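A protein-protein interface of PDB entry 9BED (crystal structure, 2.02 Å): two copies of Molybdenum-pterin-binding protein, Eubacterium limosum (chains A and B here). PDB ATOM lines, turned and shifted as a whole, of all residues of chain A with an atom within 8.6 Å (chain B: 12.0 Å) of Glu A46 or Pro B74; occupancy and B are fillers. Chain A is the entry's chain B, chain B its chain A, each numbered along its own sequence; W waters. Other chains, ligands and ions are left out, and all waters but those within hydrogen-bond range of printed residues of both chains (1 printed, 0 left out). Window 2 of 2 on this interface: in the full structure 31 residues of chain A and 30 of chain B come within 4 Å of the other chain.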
ATOM      1  N   ILE A  39       3.357 -15.409 -21.515  1.00  0.00           N
ATOM      2  CA  ILE A  39       2.889 -14.125 -21.018  1.00  0.00           C
ATOM      3  C   ILE A  39       1.377 -14.085 -21.178  1.00  0.00           C
ATOM      4  O   ILE A  39       0.787 -14.918 -21.866  1.00  0.00           O
ATOM      5  CB  ILE A  39       3.541 -12.944 -21.768  1.00  0.00           C
ATOM      6  CG1 ILE A  39       3.344 -13.143 -23.275  1.00  0.00           C
ATOM      7  CG2 ILE A  39       4.998 -12.847 -21.390  1.00  0.00           C
ATOM      8  CD1 ILE A  39       3.695 -11.918 -24.092  1.00  0.00           C
ATOM      9  N   SER A  40       0.754 -13.072 -20.572  1.00  0.00           N
ATOM     10  CA  SER A  40      -0.706 -12.992 -20.584  1.00  0.00           C
ATOM     11  C   SER A  40      -1.214 -12.687 -21.987  1.00  0.00           C
ATOM     12  O   SER A  40      -0.555 -11.995 -22.766  1.00  0.00           O
ATOM     13  CB  SER A  40      -1.213 -11.921 -19.614  1.00  0.00           C
ATOM     14  OG  SER A  40      -0.938 -10.602 -20.071  1.00  0.00           O
ATOM     15  N   MET A  41      -2.404 -13.232 -22.317  1.00  0.00           N
ATOM     16  CA  MET A  41      -3.052 -12.907 -23.592  1.00  0.00           C
ATOM     17  C   MET A  41      -3.350 -11.420 -23.704  1.00  0.00           C
ATOM     18  O   MET A  41      -3.317 -10.852 -24.810  1.00  0.00           O
ATOM     19  CB  MET A  41      -4.346 -13.699 -23.760  1.00  0.00           C
ATOM     20  CG  MET A  41      -4.209 -15.177 -24.083  1.00  0.00           C
ATOM     21  SD  MET A  41      -3.142 -15.629 -25.514  1.00  0.00           S
ATOM     22  CE  MET A  41      -3.670 -14.430 -26.734  1.00  0.00           C
ATOM     23  N   ASP A  42      -3.694 -10.775 -22.582  1.00  0.00           N
ATOM     24  CA  ASP A  42      -3.902  -9.330 -22.606  1.00  0.00           C
ATOM     25  C   ASP A  42      -2.669  -8.617 -23.154  1.00  0.00           C
ATOM     26  O   ASP A  42      -2.782  -7.757 -24.025  1.00  0.00           O
ATOM     27  CB  ASP A  42      -4.249  -8.801 -21.204  1.00  0.00           C
ATOM     28  CG  ASP A  42      -5.648  -9.251 -20.714  1.00  0.00           C
ATOM     29  OD1 ASP A  42      -6.585  -9.307 -21.530  1.00  0.00           O
ATOM     30  OD2 ASP A  42      -5.783  -9.606 -19.517  1.00  0.00           O
ATOM     31  N   SER A  43      -1.481  -9.026 -22.727  1.00  0.00           N
ATOM     32  CA  SER A  43      -0.272  -8.338 -23.165  1.00  0.00           C
ATOM     33  C   SER A  43       0.022  -8.622 -24.638  1.00  0.00           C
ATOM     34  O   SER A  43       0.452  -7.725 -25.379  1.00  0.00           O
ATOM     35  CB  SER A  43       0.906  -8.761 -22.292  1.00  0.00           C
ATOM     36  OG  SER A  43       1.469  -9.991 -22.785  1.00  0.00           O
ATOM     37  N   ILE A  44      -0.203  -9.868 -25.084  1.00  0.00           N
ATOM     38  CA  ILE A  44      -0.039 -10.201 -26.495  1.00  0.00           C
ATOM     39  C   ILE A  44      -0.910  -9.296 -27.350  1.00  0.00           C
ATOM     40  O   ILE A  44      -0.471  -8.781 -28.387  1.00  0.00           O
ATOM     41  CB  ILE A  44      -0.371 -11.690 -26.721  1.00  0.00           C
ATOM     42  CG1 ILE A  44       0.724 -12.568 -26.094  1.00  0.00           C
ATOM     43  CG2 ILE A  44      -0.459 -11.988 -28.215  1.00  0.00           C
ATOM     44  CD1 ILE A  44       0.364 -14.024 -25.946  1.00  0.00           C
ATOM     45  N   ARG A  45      -2.150  -9.072 -26.920  1.00  0.00           N
ATOM     46  CA  ARG A  45      -3.018  -8.156 -27.654  1.00  0.00           C
ATOM     47  C   ARG A  45      -2.539  -6.712 -27.564  1.00  0.00           C
ATOM     48  O   ARG A  45      -2.446  -6.018 -28.586  1.00  0.00           O
ATOM     49  CB  ARG A  45      -4.458  -8.248 -27.142  1.00  0.00           C
ATOM     50  CG  ARG A  45      -5.224  -9.473 -27.561  1.00  0.00           C
ATOM     51  CD  ARG A  45      -6.713  -9.452 -27.114  1.00  0.00           C
ATOM     52  NE  ARG A  45      -6.871  -9.609 -25.668  1.00  0.00           N
ATOM     53  CZ  ARG A  45      -7.039 -10.784 -25.068  1.00  0.00           C
ATOM     54  NH1 ARG A  45      -7.034 -11.918 -25.755  1.00  0.00           N
ATOM     55  NH2 ARG A  45      -7.206 -10.827 -23.744  1.00  0.00           N
ATOM     56  N   GLU A  46      -2.224  -6.236 -26.354  1.00  0.00           N
ATOM     57  CA  GLU A  46      -1.917  -4.816 -26.175  1.00  0.00           C
ATOM     58  C   GLU A  46      -0.650  -4.416 -26.916  1.00  0.00           C
ATOM     59  O   GLU A  46      -0.552  -3.288 -27.390  1.00  0.00           O
ATOM     60  CB  GLU A  46      -1.762  -4.470 -24.696  1.00  0.00           C
ATOM     61  CG  GLU A  46      -3.041  -4.577 -23.923  1.00  0.00           C
ATOM     62  CD  GLU A  46      -2.862  -4.393 -22.418  1.00  0.00           C
ATOM     63  OE1 GLU A  46      -1.795  -3.921 -21.972  1.00  0.00           O
ATOM     64  OE2 GLU A  46      -3.786  -4.779 -21.668  1.00  0.00           O
ATOM     65  N   LEU A  47       0.326  -5.317 -27.004  1.00  0.00           N
ATOM     66  CA  LEU A  47       1.551  -5.081 -27.749  1.00  0.00           C
ATOM     67  C   LEU A  47       1.378  -5.316 -29.246  1.00  0.00           C
ATOM     68  O   LEU A  47       2.334  -5.120 -29.994  1.00  0.00           O
ATOM     69  CB  LEU A  47       2.637  -6.004 -27.226  1.00  0.00           C
ATOM     70  CG  LEU A  47       3.076  -5.848 -25.771  1.00  0.00           C
ATOM     71  CD1 LEU A  47       4.022  -7.023 -25.420  1.00  0.00           C
ATOM     72  CD2 LEU A  47       3.777  -4.550 -25.540  1.00  0.00           C
ATOM     73  N   GLY A  48       0.196  -5.733 -29.696  1.00  0.00           N
ATOM     74  CA  GLY A  48      -0.042  -5.933 -31.122  1.00  0.00           C
ATOM     75  C   GLY A  48       0.788  -7.022 -31.764  1.00  0.00           C
ATOM     76  O   GLY A  48       1.084  -6.948 -32.962  1.00  0.00           O
ATOM     77  N   LEU A  49       1.163  -8.046 -31.005  1.00  0.00           N
ATOM     78  CA  LEU A  49       2.074  -9.049 -31.538  1.00  0.00           C
ATOM     79  C   LEU A  49       1.400  -9.933 -32.578  1.00  0.00           C
ATOM     80  O   LEU A  49       0.308 -10.463 -32.357  1.00  0.00           O
ATOM     81  CB  LEU A  49       2.637  -9.924 -30.418  1.00  0.00           C
ATOM     82  CG  LEU A  49       3.442  -9.256 -29.305  1.00  0.00           C
ATOM     83  CD1 LEU A  49       3.844 -10.302 -28.299  1.00  0.00           C
ATOM     84  CD2 LEU A  49       4.656  -8.610 -29.878  1.00  0.00           C
ATOM     85  N   SER A  53       6.162  -9.839 -36.327  1.00  0.00           N
ATOM     86  CA  SER A  53       6.447  -8.620 -35.569  1.00  0.00           C
ATOM     87  C   SER A  53       7.887  -8.605 -35.073  1.00  0.00           C
ATOM     88  O   SER A  53       8.443  -9.642 -34.712  1.00  0.00           O
ATOM     89  CB  SER A  53       5.539  -8.486 -34.340  1.00  0.00           C
ATOM     90  OG  SER A  53       4.169  -8.424 -34.653  1.00  0.00           O
ATOM     91  N   ILE B  66       7.980 -10.010 -23.162  1.00  0.00           N
ATOM     92  CA  ILE B  66       8.140  -9.496 -24.512  1.00  0.00           C
ATOM     93  C   ILE B  66       8.071  -7.979 -24.467  1.00  0.00           C
ATOM     94  O   ILE B  66       7.207  -7.405 -23.793  1.00  0.00           O
ATOM     95  CB  ILE B  66       7.080 -10.040 -25.496  1.00  0.00           C
ATOM     96  CG1 ILE B  66       7.158 -11.585 -25.640  1.00  0.00           C
ATOM     97  CG2 ILE B  66       7.264  -9.346 -26.859  1.00  0.00           C
ATOM     98  CD1 ILE B  66       8.461 -12.106 -26.279  1.00  0.00           C
ATOM     99  N   GLY B  67       8.970  -7.337 -25.199  1.00  0.00           N
ATOM    100  CA  GLY B  67       8.908  -5.900 -25.398  1.00  0.00           C
ATOM    101  C   GLY B  67       8.814  -5.509 -26.866  1.00  0.00           C
ATOM    102  O   GLY B  67       9.173  -6.301 -27.746  1.00  0.00           O
ATOM    103  N   ILE B  68       8.336  -4.293 -27.140  1.00  0.00           N
ATOM    104  CA  ILE B  68       8.316  -3.721 -28.480  1.00  0.00           C
ATOM    105  C   ILE B  68       8.891  -2.313 -28.374  1.00  0.00           C
ATOM    106  O   ILE B  68       8.984  -1.735 -27.290  1.00  0.00           O
ATOM    107  CB  ILE B  68       6.904  -3.700 -29.112  1.00  0.00           C
ATOM    108  CG1 ILE B  68       5.952  -2.829 -28.290  1.00  0.00           C
ATOM    109  CG2 ILE B  68       6.362  -5.117 -29.281  1.00  0.00           C
ATOM    110  CD1 ILE B  68       4.593  -2.631 -28.933  1.00  0.00           C
ATOM    111  N   ASP B  69       9.290  -1.760 -29.513  1.00  0.00           N
ATOM    112  CA  ASP B  69       9.804  -0.389 -29.515  1.00  0.00           C
ATOM    113  C   ASP B  69       8.745   0.663 -29.160  1.00  0.00           C
ATOM    114  O   ASP B  69       7.541   0.484 -29.364  1.00  0.00           O
ATOM    115  CB  ASP B  69      10.405  -0.041 -30.876  1.00  0.00           C
ATOM    116  CG  ASP B  69      11.745  -0.707 -31.117  1.00  0.00           C
ATOM    117  OD1 ASP B  69      12.581  -0.733 -30.185  1.00  0.00           O
ATOM    118  OD2 ASP B  69      11.946  -1.202 -32.238  1.00  0.00           O
ATOM    119  N   ASP B  70       9.229   1.807 -28.661  1.00  0.00           N
ATOM    120  CA  ASP B  70       8.323   2.840 -28.170  1.00  0.00           C
ATOM    121  C   ASP B  70       7.437   3.383 -29.276  1.00  0.00           C
ATOM    122  O   ASP B  70       6.336   3.866 -29.009  1.00  0.00           O
ATOM    123  CB  ASP B  70       9.103   4.026 -27.573  1.00  0.00           C
ATOM    124  CG  ASP B  70       9.901   3.686 -26.323  1.00  0.00           C
ATOM    125  OD1 ASP B  70       9.545   2.743 -25.601  1.00  0.00           O
ATOM    126  OD2 ASP B  70      10.888   4.423 -26.053  1.00  0.00           O
ATOM    127  N   TRP B  71       7.922   3.391 -30.513  1.00  0.00           N
ATOM    128  CA  TRP B  71       7.186   3.998 -31.618  1.00  0.00           C
ATOM    129  C   TRP B  71       6.284   3.011 -32.351  1.00  0.00           C
ATOM    130  O   TRP B  71       5.712   3.357 -33.395  1.00  0.00           O
ATOM    131  CB  TRP B  71       8.162   4.631 -32.601  1.00  0.00           C
ATOM    132  CG  TRP B  71       9.204   3.675 -33.061  1.00  0.00           C
ATOM    133  CD1 TRP B  71       9.128   2.818 -34.123  1.00  0.00           C
ATOM    134  CD2 TRP B  71      10.478   3.467 -32.465  1.00  0.00           C
ATOM    135  NE1 TRP B  71      10.283   2.095 -34.223  1.00  0.00           N
ATOM    136  CE2 TRP B  71      11.129   2.474 -33.212  1.00  0.00           C
ATOM    137  CE3 TRP B  71      11.130   4.010 -31.348  1.00  0.00           C
ATOM    138  CZ2 TRP B  71      12.404   2.026 -32.890  1.00  0.00           C
ATOM    139  CZ3 TRP B  71      12.396   3.561 -31.042  1.00  0.00           C
ATOM    140  CH2 TRP B  71      13.028   2.608 -31.823  1.00  0.00           C
ATOM    141  N   SER B  72       6.149   1.789 -31.844  1.00  0.00           N
ATOM    142  CA  SER B  72       5.111   0.894 -32.333  1.00  0.00           C
ATOM    143  C   SER B  72       3.793   1.258 -31.652  1.00  0.00           C
ATOM    144  O   SER B  72       3.765   1.445 -30.437  1.00  0.00           O
ATOM    145  CB  SER B  72       5.485  -0.560 -32.058  1.00  0.00           C
ATOM    146  OG  SER B  72       4.383  -1.390 -32.368  1.00  0.00           O
ATOM    147  N   HIS B  73       2.701   1.389 -32.421  1.00  0.00           N
ATOM    148  CA  HIS B  73       1.405   1.818 -31.875  1.00  0.00           C
ATOM    149  C   HIS B  73       0.325   0.755 -32.091  1.00  0.00           C
ATOM    150  O   HIS B  73      -0.595   0.938 -32.902  1.00  0.00           O
ATOM    151  CB  HIS B  73       0.914   3.137 -32.476  1.00  0.00           C
ATOM    152  CG  HIS B  73       1.956   4.200 -32.554  1.00  0.00           C
ATOM    153  ND1 HIS B  73       2.725   4.566 -31.470  1.00  0.00           N
ATOM    154  CD2 HIS B  73       2.353   4.987 -33.584  1.00  0.00           C
ATOM    155  CE1 HIS B  73       3.564   5.522 -31.832  1.00  0.00           C
ATOM    156  NE2 HIS B  73       3.364   5.792 -33.111  1.00  0.00           N
ATOM    157  N   PRO B  74       0.365  -0.347 -31.334  1.00  0.00           N
ATOM    158  CA  PRO B  74      -0.666  -1.393 -31.519  1.00  0.00           C
ATOM    159  C   PRO B  74      -2.110  -0.916 -31.306  1.00  0.00           C
ATOM    160  O   PRO B  74      -2.343  -0.090 -30.415  1.00  0.00           O
ATOM    161  CB  PRO B  74      -0.302  -2.458 -30.470  1.00  0.00           C
ATOM    162  CG  PRO B  74       0.688  -1.780 -29.508  1.00  0.00           C
ATOM    163  CD  PRO B  74       1.371  -0.686 -30.310  1.00  0.00           C
HETATM  164  O   HOH W   1       4.053  -4.751 -32.299  1.00  0.00           O
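Water W1 lies within hydrogen-bond range of the backbone carbonyl oxygen (O) of Leu A47 (2.9 Å) and the side-chain hydroxyl (OG) of Ser B72 (3.4 Å).
Among the printed residues, merely in contact across the chains: Glu A46 with Pro B74 (2.9 Å), Gly A48 with Pro B74 (3.4 Å), Leu A47 with Ile B68 (3.5 Å), Leu A47 with Pro B74 (3.5 Å), Leu A47 with Ile B66 (3.6 Å), Ile A39 with Ile B66 (3.8 Å), Leu A49 with Ile B66 (3.8 Å) and Leu A49 with Ile B68 (3.9 Å).
Printed residues of chain B within 4 Å of Ile A39: Ile B66 (3.8 Å).
No residue of chain B comes within 4 Å of Ser A43.
No residue of chain B comes within 4 Å of Arg A45.
Glu A46 touches one residue of chain B.
Of chain B, only Ile B66, Ile B68 and Pro B74 come within 4 Å of Leu A47.
Of chain B, only Pro B74 comes within 4 Å of Gly A48.
Of the printed residues of chain B, Leu A49 touches Ile B66 and Ile B68.
Ser A53 touches none of the printed residues of chain B.
Gly B67 touches none of the printed residues of chain A.
Of the printed residues of chain A, Ile B68 touches Leu A47 (3.5 Å) and Leu A49 (3.9 Å).
Pro B74 touches just these residues of chain A: Glu A46, Leu A47 and Gly A48.
The nearest residue of chain B that does not touch Glu A46 is Ile B68 (5.4 Å).
The nearest printed residue of chain B that does not touch Ile A39 is Gly B67 (7.1 Å).
Hydrophobic or aromatic side chains of chain B that line the printed part of chain A: Ile B66, Ile B68 and Pro B74.
Of the 12 printed residues of chain A, 5 touch a printed residue of chain B.
No position is printed for both chains.
Of the 8 pairs that touch across the chains among the printed residues, none has its exchanged pair printed and touching as well.
The backbone NH (N) of Leu A49 sits at hydrogen-bond distance from the backbone carbonyl oxygen (O) of Ile A44 (3.2 Å).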
